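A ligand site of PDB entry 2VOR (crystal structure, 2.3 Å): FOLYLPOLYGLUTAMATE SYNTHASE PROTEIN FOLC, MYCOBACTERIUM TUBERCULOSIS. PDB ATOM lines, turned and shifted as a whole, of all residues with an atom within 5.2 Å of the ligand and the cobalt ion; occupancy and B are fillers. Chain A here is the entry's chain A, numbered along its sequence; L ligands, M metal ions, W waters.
Pro 99 touches the cobalt ion (CD to CO, 3.9 Å).
Within 4 Å of the cobalt ion: Thr 76, Ser 98, Pro 99 and Glu 174.
An oxygen (O8) of the ligand sits at hydrogen-bond distance from the backbone NH of Gly 74, 2.9 Å away.
O7 of the ligand lies within hydrogen-bond range of N of Ser 77, 3.3 Å away.
An oxygen (O3) of the ligand sits at hydrogen-bond distance from a ring nitrogen (NE2) of His 354, at 3.0 Å.
An oxygen (O4) of the ligand lies within salt-bridge range of the side-chain amino group of Lys 75.
An oxygen (O7) of the ligand lies within hydrogen-bond range of the side-chain hydroxyl of Ser 77 (2.6 Å).
An oxygen (O10) of the ligand lies within hydrogen-bond range of the side-chain amide nitrogen of Asn 73, 3.4 Å away.
O11 of the ligand lies within hydrogen-bond range of OD1 of Asp 351 (2.8 Å).
ND2 of Asn 301 sits at hydrogen-bond distance from N2 of the ligand (3.0 Å).
The backbone NH of Lys 75 lies within hydrogen-bond range of an oxygen (O4) of the ligand, at 3.0 Å.
O of Thr 72 sits close to O4 of the ligand, 3.0 Å away.
The backbone NH of Ala 352 lies within hydrogen-bond range of an oxygen (O11) of the ligand (3.4 Å).
N of Thr 76 lies close to O5 of the ligand (2.8 Å).
The guanidinium group (NE) of Arg 338 is in salt-bridge range of an oxygen (O6) of the ligand (2.7 Å).
Water W3 lies within hydrogen-bond range of a ring nitrogen (NE2) of His 354, the side-chain amide nitrogen of Asn 73 and the backbone carbonyl oxygen of Thr 72.
Water W2 lies within hydrogen-bond range of N of His 354, ND2 of Asn 73 and O10 of the ligand.
Water W4 bridges NE2 of His 297 (2.7 Å) and NE2 of Gln 298 (3.3 Å).
The cobalt ion is bound by an oxygen (O1) of the ligand (2.0 Å), an oxygen (O5) of the ligand (2.1 Å), the backbone carbonyl oxygen of Ser 98 (2.2 Å), the side-chain carboxylate of Glu 174 (2.2 Å) and the side-chain hydroxyl of Thr 76 (2.4 Å).
The cobalt ion has five donor atoms within binding distance.
Merely in contact with the ligand: Pro 99, His 297, Ala 353, Gly 358, Ala 361 and Val 472.
Within 4 Å of the ligand: Thr 72, Asn 73, Gly 74, Lys 75, Thr 76, Ser 77, Ser 98, Pro 99, Glu 174, His 297, Asn 301, Arg 338, Asp 351, Ala 352, Ala 353, His 354, Gly 358, Ala 361 and Val 472.
O of Pro 196 lies within hydrogen-bond range of N of Asn 73.
ND2 of Asn 301 sits at hydrogen-bond distance from OE1 of Gln 298 (3.0 Å).
N of Leu 339 sits at hydrogen-bond distance from OD1 of Asp 351 (2.8 Å).
OG of Ser 77 is in hydrogen-bond range of NE2 of Gln 298 (3.5 Å).
The side-chain amino group (NZ) of Lys 75 sits at hydrogen-bond distance from the backbone carbonyl oxygen (O) of Gly 71 (3.2 Å).
The backbone NH of Thr 72 is in hydrogen-bond range of the backbone carbonyl oxygen of Pro 196, at 2.9 Å.
OD2 of Asp 351 sits at hydrogen-bond distance from N of Ala 353, 3.0 Å away.
O of Gly 337 lies within hydrogen-bond range of N of Ala 352.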
ATOM      1  N   GLY A  71       8.438 -20.418 -23.554  1.00  0.00           N
ATOM      2  CA  GLY A  71       8.698 -20.462 -25.014  1.00  0.00           C
ATOM      3  C   GLY A  71       9.824 -21.436 -25.173  1.00  0.00           C
ATOM      4  O   GLY A  71      10.330 -21.974 -24.181  1.00  0.00           O
ATOM      5  N   THR A  72      10.244 -21.683 -26.405  1.00  0.00           N
ATOM      6  CA  THR A  72      11.313 -22.630 -26.616  1.00  0.00           C
ATOM      7  C   THR A  72      12.662 -21.921 -26.752  1.00  0.00           C
ATOM      8  O   THR A  72      13.692 -22.356 -26.205  1.00  0.00           O
ATOM      9  CB  THR A  72      11.082 -23.486 -27.927  1.00  0.00           C
ATOM     10  OG1 THR A  72       9.806 -24.171 -27.823  1.00  0.00           O
ATOM     11  CG2 THR A  72      12.181 -24.502 -28.132  1.00  0.00           C
ATOM     12  N   ASN A  73      12.680 -20.863 -27.521  1.00  0.00           N
ATOM     13  CA  ASN A  73      13.903 -20.144 -27.768  1.00  0.00           C
ATOM     14  C   ASN A  73      13.772 -18.655 -27.427  1.00  0.00           C
ATOM     15  O   ASN A  73      12.730 -18.014 -27.737  1.00  0.00           O
ATOM     16  CB  ASN A  73      14.236 -20.234 -29.206  1.00  0.00           C
ATOM     17  CG  ASN A  73      14.829 -21.605 -29.592  1.00  0.00           C
ATOM     18  OD1 ASN A  73      14.306 -22.249 -30.518  1.00  0.00           O
ATOM     19  ND2 ASN A  73      15.977 -22.012 -28.950  1.00  0.00           N
ATOM     20  N   GLY A  74      14.849 -18.088 -26.835  1.00  0.00           N
ATOM     21  CA  GLY A  74      14.944 -16.674 -26.664  1.00  0.00           C
ATOM     22  C   GLY A  74      14.434 -16.335 -25.325  1.00  0.00           C
ATOM     23  O   GLY A  74      14.387 -15.210 -25.011  1.00  0.00           O
ATOM     24  N   LYS A  75      14.086 -17.272 -24.482  1.00  0.00           N
ATOM     25  CA  LYS A  75      13.528 -16.813 -23.224  1.00  0.00           C
ATOM     26  C   LYS A  75      14.521 -16.013 -22.403  1.00  0.00           C
ATOM     27  O   LYS A  75      14.158 -15.020 -21.720  1.00  0.00           O
ATOM     28  CB  LYS A  75      12.968 -17.949 -22.318  1.00  0.00           C
ATOM     29  CG  LYS A  75      12.056 -18.995 -22.952  1.00  0.00           C
ATOM     30  CD  LYS A  75      11.517 -19.983 -21.794  1.00  0.00           C
ATOM     31  CE  LYS A  75      12.657 -20.983 -21.418  1.00  0.00           C
ATOM     32  NZ  LYS A  75      13.187 -21.605 -22.745  1.00  0.00           N
ATOM     33  N   THR A  76      15.750 -16.527 -22.341  1.00  0.00           N
ATOM     34  CA  THR A  76      16.827 -15.845 -21.559  1.00  0.00           C
ATOM     35  C   THR A  76      17.191 -14.478 -22.084  1.00  0.00           C
ATOM     36  O   THR A  76      17.224 -13.561 -21.353  1.00  0.00           O
ATOM     37  CB  THR A  76      18.120 -16.682 -21.384  1.00  0.00           C
ATOM     38  OG1 THR A  76      17.858 -17.626 -20.369  1.00  0.00           O
ATOM     39  CG2 THR A  76      19.302 -15.758 -20.872  1.00  0.00           C
ATOM     40  N   SER A  77      17.423 -14.393 -23.382  1.00  0.00           N
ATOM     41  CA  SER A  77      17.598 -13.168 -24.045  1.00  0.00           C
ATOM     42  C   SER A  77      16.520 -12.109 -23.807  1.00  0.00           C
ATOM     43  O   SER A  77      16.873 -10.958 -23.589  1.00  0.00           O
ATOM     44  CB  SER A  77      17.681 -13.413 -25.516  1.00  0.00           C
ATOM     45  OG  SER A  77      18.826 -14.160 -25.741  1.00  0.00           O
ATOM     46  N   SER A  98      17.351 -19.175 -16.475  1.00  0.00           N
ATOM     47  CA  SER A  98      17.921 -20.530 -16.460  1.00  0.00           C
ATOM     48  C   SER A  98      18.100 -21.012 -17.855  1.00  0.00           C
ATOM     49  O   SER A  98      17.555 -20.401 -18.805  1.00  0.00           O
ATOM     50  CB  SER A  98      17.093 -21.546 -15.653  1.00  0.00           C
ATOM     51  OG  SER A  98      15.781 -21.609 -16.155  1.00  0.00           O
ATOM     52  N   PRO A  99      18.970 -22.042 -18.016  1.00  0.00           N
ATOM     53  CA  PRO A  99      19.899 -22.468 -16.942  1.00  0.00           C
ATOM     54  C   PRO A  99      21.093 -21.495 -16.785  1.00  0.00           C
ATOM     55  O   PRO A  99      21.256 -20.636 -17.642  1.00  0.00           O
ATOM     56  CB  PRO A  99      20.485 -23.807 -17.482  1.00  0.00           C
ATOM     57  CG  PRO A  99      20.331 -23.780 -18.939  1.00  0.00           C
ATOM     58  CD  PRO A  99      19.288 -22.641 -19.333  1.00  0.00           C
ATOM     59  N   GLU A 174      11.831 -16.102 -15.908  1.00  0.00           N
ATOM     60  CA  GLU A 174      11.908 -17.153 -16.884  1.00  0.00           C
ATOM     61  C   GLU A 174      11.479 -18.547 -16.337  1.00  0.00           C
ATOM     62  O   GLU A 174      11.858 -18.994 -15.240  1.00  0.00           O
ATOM     63  CB  GLU A 174      13.351 -17.212 -17.424  1.00  0.00           C
ATOM     64  CG  GLU A 174      13.541 -18.267 -18.411  1.00  0.00           C
ATOM     65  CD  GLU A 174      14.969 -18.350 -18.910  1.00  0.00           C
ATOM     66  OE1 GLU A 174      15.869 -17.498 -18.564  1.00  0.00           O
ATOM     67  OE2 GLU A 174      15.182 -19.295 -19.679  1.00  0.00           O
ATOM     68  N   PRO A 196       9.190 -17.751 -29.409  1.00  0.00           N
ATOM     69  CA  PRO A 196       8.869 -18.808 -30.384  1.00  0.00           C
ATOM     70  C   PRO A 196       8.957 -20.243 -29.824  1.00  0.00           C
ATOM     71  O   PRO A 196       9.887 -20.586 -29.077  1.00  0.00           O
ATOM     72  CB  PRO A 196       9.851 -18.550 -31.497  1.00  0.00           C
ATOM     73  CG  PRO A 196      10.055 -16.999 -31.461  1.00  0.00           C
ATOM     74  CD  PRO A 196      10.053 -16.700 -29.978  1.00  0.00           C
ATOM     75  N   HIS A 297      17.188 -13.075 -35.297  1.00  0.00           N
ATOM     76  CA  HIS A 297      16.412 -13.552 -34.192  1.00  0.00           C
ATOM     77  C   HIS A 297      16.440 -12.608 -32.975  1.00  0.00           C
ATOM     78  O   HIS A 297      15.439 -12.500 -32.237  1.00  0.00           O
ATOM     79  CB  HIS A 297      16.818 -14.999 -33.792  1.00  0.00           C
ATOM     80  CG  HIS A 297      18.244 -15.141 -33.345  1.00  0.00           C
ATOM     81  ND1 HIS A 297      19.310 -15.056 -34.214  1.00  0.00           N
ATOM     82  CD2 HIS A 297      18.766 -15.385 -32.127  1.00  0.00           C
ATOM     83  CE1 HIS A 297      20.435 -15.220 -33.547  1.00  0.00           C
ATOM     84  NE2 HIS A 297      20.132 -15.411 -32.276  1.00  0.00           N
ATOM     85  N   GLN A 298      17.549 -11.891 -32.767  1.00  0.00           N
ATOM     86  CA  GLN A 298      17.637 -11.010 -31.614  1.00  0.00           C
ATOM     87  C   GLN A 298      16.811  -9.732 -31.874  1.00  0.00           C
ATOM     88  O   GLN A 298      16.408  -9.080 -30.944  1.00  0.00           O
ATOM     89  CB  GLN A 298      19.122 -10.683 -31.223  1.00  0.00           C
ATOM     90  CG  GLN A 298      19.921 -11.871 -30.714  1.00  0.00           C
ATOM     91  CD  GLN A 298      19.495 -12.304 -29.325  1.00  0.00           C
ATOM     92  OE1 GLN A 298      18.458 -11.904 -28.817  1.00  0.00           O
ATOM     93  NE2 GLN A 298      20.300 -13.145 -28.695  1.00  0.00           N
ATOM     94  N   ASN A 301      13.455 -11.004 -30.586  1.00  0.00           N
ATOM     95  CA  ASN A 301      13.526 -10.926 -29.122  1.00  0.00           C
ATOM     96  C   ASN A 301      13.406  -9.472 -28.652  1.00  0.00           C
ATOM     97  O   ASN A 301      12.637  -9.162 -27.749  1.00  0.00           O
ATOM     98  CB  ASN A 301      14.830 -11.613 -28.564  1.00  0.00           C
ATOM     99  CG  ASN A 301      14.871 -13.139 -28.837  1.00  0.00           C
ATOM    100  OD1 ASN A 301      13.808 -13.747 -29.001  1.00  0.00           O
ATOM    101  ND2 ASN A 301      16.074 -13.745 -28.862  1.00  0.00           N
ATOM    102  N   SER A 335      23.930 -10.535 -23.516  1.00  0.00           N
ATOM    103  CA  SER A 335      23.399 -11.900 -23.473  1.00  0.00           C
ATOM    104  C   SER A 335      24.569 -12.838 -23.608  1.00  0.00           C
ATOM    105  O   SER A 335      24.890 -13.290 -24.667  1.00  0.00           O
ATOM    106  CB  SER A 335      22.392 -12.152 -24.596  1.00  0.00           C
ATOM    107  OG  SER A 335      21.576 -13.319 -24.309  1.00  0.00           O
ATOM    108  N   GLY A 337      27.163 -15.804 -23.842  1.00  0.00           N
ATOM    109  CA  GLY A 337      27.058 -17.137 -24.478  1.00  0.00           C
ATOM    110  C   GLY A 337      25.989 -17.260 -25.547  1.00  0.00           C
ATOM    111  O   GLY A 337      25.680 -18.354 -25.995  1.00  0.00           O
ATOM    112  N   ARG A 338      25.377 -16.154 -25.941  1.00  0.00           N
ATOM    113  CA  ARG A 338      24.536 -16.110 -27.172  1.00  0.00           C
ATOM    114  C   ARG A 338      25.278 -15.272 -28.247  1.00  0.00           C
ATOM    115  O   ARG A 338      25.408 -14.021 -28.123  1.00  0.00           O
ATOM    116  CB  ARG A 338      23.135 -15.531 -26.881  1.00  0.00           C
ATOM    117  CG  ARG A 338      22.172 -16.515 -26.151  1.00  0.00           C
ATOM    118  CD  ARG A 338      22.755 -16.867 -24.744  1.00  0.00           C
ATOM    119  NE  ARG A 338      21.883 -17.599 -23.810  1.00  0.00           N
ATOM    120  CZ  ARG A 338      22.180 -17.942 -22.548  1.00  0.00           C
ATOM    121  NH1 ARG A 338      23.338 -17.594 -21.969  1.00  0.00           N
ATOM    122  NH2 ARG A 338      21.313 -18.629 -21.816  1.00  0.00           N
ATOM    123  N   LEU A 339      25.837 -15.962 -29.229  1.00  0.00           N
ATOM    124  CA  LEU A 339      26.722 -15.369 -30.252  1.00  0.00           C
ATOM    125  C   LEU A 339      27.621 -14.260 -29.647  1.00  0.00           C
ATOM    126  O   LEU A 339      27.594 -13.084 -30.059  1.00  0.00           O
ATOM    127  CB  LEU A 339      25.868 -14.797 -31.335  1.00  0.00           C
ATOM    128  CG  LEU A 339      26.051 -15.187 -32.807  1.00  0.00           C
ATOM    129  CD1 LEU A 339      27.246 -16.015 -33.026  1.00  0.00           C
ATOM    130  CD2 LEU A 339      24.746 -15.808 -33.307  1.00  0.00           C
ATOM    131  N   ASP A 351      28.197 -19.851 -28.645  1.00  0.00           N
ATOM    132  CA  ASP A 351      26.749 -19.715 -28.775  1.00  0.00           C
ATOM    133  C   ASP A 351      26.028 -20.886 -28.191  1.00  0.00           C
ATOM    134  O   ASP A 351      26.425 -21.991 -28.382  1.00  0.00           O
ATOM    135  CB  ASP A 351      26.306 -19.461 -30.202  1.00  0.00           C
ATOM    136  CG  ASP A 351      24.769 -19.247 -30.295  1.00  0.00           C
ATOM    137  OD1 ASP A 351      24.252 -18.150 -29.994  1.00  0.00           O
ATOM    138  OD2 ASP A 351      24.056 -20.222 -30.634  1.00  0.00           O
ATOM    139  N   ALA A 352      24.957 -20.654 -27.441  1.00  0.00           N
ATOM    140  CA  ALA A 352      24.343 -21.705 -26.638  1.00  0.00           C
ATOM    141  C   ALA A 352      23.345 -22.515 -27.442  1.00  0.00           C
ATOM    142  O   ALA A 352      22.490 -23.163 -26.840  1.00  0.00           O
ATOM    143  CB  ALA A 352      23.614 -21.049 -25.349  1.00  0.00           C
ATOM    144  N   ALA A 353      23.400 -22.468 -28.777  1.00  0.00           N
ATOM    145  CA  ALA A 353      22.410 -23.169 -29.660  1.00  0.00           C
ATOM    146  C   ALA A 353      22.321 -24.658 -29.363  1.00  0.00           C
ATOM    147  O   ALA A 353      23.291 -25.366 -29.470  1.00  0.00           O
ATOM    148  CB  ALA A 353      22.743 -22.952 -31.136  1.00  0.00           C
ATOM    149  N   HIS A 354      21.164 -25.137 -28.964  1.00  0.00           N
ATOM    150  CA  HIS A 354      21.034 -26.532 -28.578  1.00  0.00           C
ATOM    151  C   HIS A 354      19.772 -27.192 -29.134  1.00  0.00           C
ATOM    152  O   HIS A 354      19.315 -28.199 -28.625  1.00  0.00           O
ATOM    153  CB  HIS A 354      21.135 -26.727 -27.069  1.00  0.00           C
ATOM    154  CG  HIS A 354      20.172 -25.916 -26.257  1.00  0.00           C
ATOM    155  ND1 HIS A 354      18.842 -26.280 -26.082  1.00  0.00           N
ATOM    156  CD2 HIS A 354      20.360 -24.809 -25.494  1.00  0.00           C
ATOM    157  CE1 HIS A 354      18.255 -25.413 -25.274  1.00  0.00           C
ATOM    158  NE2 HIS A 354      19.154 -24.495 -24.938  1.00  0.00           N
ATOM    159  N   ALA A 357      16.040 -25.078 -34.396  1.00  0.00           N
ATOM    160  CA  ALA A 357      15.670 -23.703 -34.655  1.00  0.00           C
ATOM    161  C   ALA A 357      16.804 -22.772 -34.192  1.00  0.00           C
ATOM    162  O   ALA A 357      17.162 -21.845 -34.904  1.00  0.00           O
ATOM    163  CB  ALA A 357      14.360 -23.381 -33.925  1.00  0.00           C
ATOM    164  N   GLY A 358      17.395 -23.021 -33.037  1.00  0.00           N
ATOM    165  CA  GLY A 358      18.548 -22.214 -32.507  1.00  0.00           C
ATOM    166  C   GLY A 358      19.794 -22.365 -33.390  1.00  0.00           C
ATOM    167  O   GLY A 358      20.460 -21.396 -33.713  1.00  0.00           O
ATOM    168  N   ALA A 359      20.094 -23.581 -33.765  1.00  0.00           N
ATOM    169  CA  ALA A 359      21.213 -23.972 -34.664  1.00  0.00           C
ATOM    170  C   ALA A 359      21.082 -23.298 -36.061  1.00  0.00           C
ATOM    171  O   ALA A 359      22.056 -22.840 -36.719  1.00  0.00           O
ATOM    172  CB  ALA A 359      21.210 -25.527 -34.787  1.00  0.00           C
ATOM    173  N   ALA A 361      19.285 -20.537 -36.596  1.00  0.00           N
ATOM    174  CA  ALA A 361      19.404 -19.085 -36.370  1.00  0.00           C
ATOM    175  C   ALA A 361      20.883 -18.730 -36.232  1.00  0.00           C
ATOM    176  O   ALA A 361      21.349 -17.759 -36.806  1.00  0.00           O
ATOM    177  CB  ALA A 361      18.571 -18.628 -35.126  1.00  0.00           C
ATOM    178  N   LEU A 362      21.644 -19.573 -35.534  1.00  0.00           N
ATOM    179  CA  LEU A 362      23.069 -19.406 -35.524  1.00  0.00           C
ATOM    180  C   LEU A 362      23.723 -19.435 -36.945  1.00  0.00           C
ATOM    181  O   LEU A 362      24.506 -18.567 -37.250  1.00  0.00           O
ATOM    182  CB  LEU A 362      23.701 -20.436 -34.582  1.00  0.00           C
ATOM    183  CG  LEU A 362      25.240 -20.500 -34.667  1.00  0.00           C
ATOM    184  CD1 LEU A 362      25.726 -19.129 -34.128  1.00  0.00           C
ATOM    185  CD2 LEU A 362      25.894 -21.712 -33.897  1.00  0.00           C
ATOM    186  N   VAL A 472      24.246 -24.982 -23.647  1.00  0.00           N
ATOM    187  CA  VAL A 472      24.461 -23.953 -22.665  1.00  0.00           C
ATOM    188  C   VAL A 472      25.683 -24.285 -21.856  1.00  0.00           C
ATOM    189  O   VAL A 472      26.473 -23.381 -21.483  1.00  0.00           O
ATOM    190  CB  VAL A 472      23.320 -23.932 -21.664  1.00  0.00           C
ATOM    191  CG1 VAL A 472      23.657 -23.040 -20.464  1.00  0.00           C
ATOM    192  CG2 VAL A 472      22.092 -23.466 -22.348  1.00  0.00           C
HETATM  193  P1  LIG L   1      18.455 -21.737 -22.917  1.00  0.00           P
HETATM  194  O1  LIG L   1      18.574 -20.209 -21.955  1.00  0.00           O
HETATM  195  O2  LIG L   1      18.148 -23.065 -22.191  1.00  0.00           O
HETATM  196  O3  LIG L   1      19.712 -21.762 -23.734  1.00  0.00           O
HETATM  197  P2  LIG L   1      16.330 -19.921 -24.086  1.00  0.00           P
HETATM  198  O4  LIG L   1      14.933 -20.148 -24.509  1.00  0.00           O
HETATM  199  O5  LIG L   1      16.340 -19.269 -22.755  1.00  0.00           O
HETATM  200  C1  LIG L   1      16.831 -21.664 -23.741  1.00  0.00           C
HETATM  201  P3  LIG L   1      18.137 -18.064 -24.999  1.00  0.00           P
HETATM  202  O6  LIG L   1      19.413 -18.639 -24.265  1.00  0.00           O
HETATM  203  O7  LIG L   1      18.185 -16.690 -25.620  1.00  0.00           O
HETATM  204  O8  LIG L   1      17.046 -19.267 -25.315  1.00  0.00           O
HETATM  205  O9  LIG L   1      18.874 -18.579 -26.469  1.00  0.00           O
HETATM  206  C2  LIG L   1      19.441 -19.944 -26.740  1.00  0.00           C
HETATM  207  C3  LIG L   1      19.963 -20.084 -28.152  1.00  0.00           C
HETATM  208  O10 LIG L   1      18.762 -19.981 -28.954  1.00  0.00           O
HETATM  209  C4  LIG L   1      20.742 -18.831 -28.548  1.00  0.00           C
HETATM  210  O11 LIG L   1      22.140 -18.981 -28.370  1.00  0.00           O
HETATM  211  C5  LIG L   1      20.447 -18.643 -30.033  1.00  0.00           C
HETATM  212  O12 LIG L   1      21.235 -19.516 -30.846  1.00  0.00           O
HETATM  213  C6  LIG L   1      19.040 -19.170 -30.150  1.00  0.00           C
HETATM  214  N1  LIG L   1      17.903 -18.203 -30.108  1.00  0.00           N
HETATM  215  C7  LIG L   1      17.638 -17.218 -29.189  1.00  0.00           C
HETATM  216  N2  LIG L   1      16.473 -16.606 -29.486  1.00  0.00           N
HETATM  217  C8  LIG L   1      16.027 -17.190 -30.617  1.00  0.00           C
HETATM  218  C9  LIG L   1      14.895 -17.011 -31.387  1.00  0.00           C
HETATM  219  N3  LIG L   1      13.999 -16.076 -31.072  1.00  0.00           N
HETATM  220  N4  LIG L   1      14.729 -17.816 -32.438  1.00  0.00           N
HETATM  221  C10 LIG L   1      15.619 -18.727 -32.801  1.00  0.00           C
HETATM  222  N5  LIG L   1      16.714 -18.940 -32.089  1.00  0.00           N
HETATM  223  C11 LIG L   1      16.912 -18.203 -30.993  1.00  0.00           C
HETATM  224 CO    CO M   1      17.027 -19.800 -20.810  1.00  0.00          CO
HETATM  225  O   HOH W   1      12.510 -18.588 -34.162  1.00  0.00           O
HETATM  226  O   HOH W   2      18.861 -23.201 -28.877  1.00  0.00           O
HETATM  227  O   HOH W   3      16.746 -23.076 -26.101  1.00  0.00           O
HETATM  228  O   HOH W   4      21.953 -15.490 -30.234  1.00  0.00           O
HETATM  229  O   HOH W   5      12.725 -15.222 -34.078  1.00  0.00           O
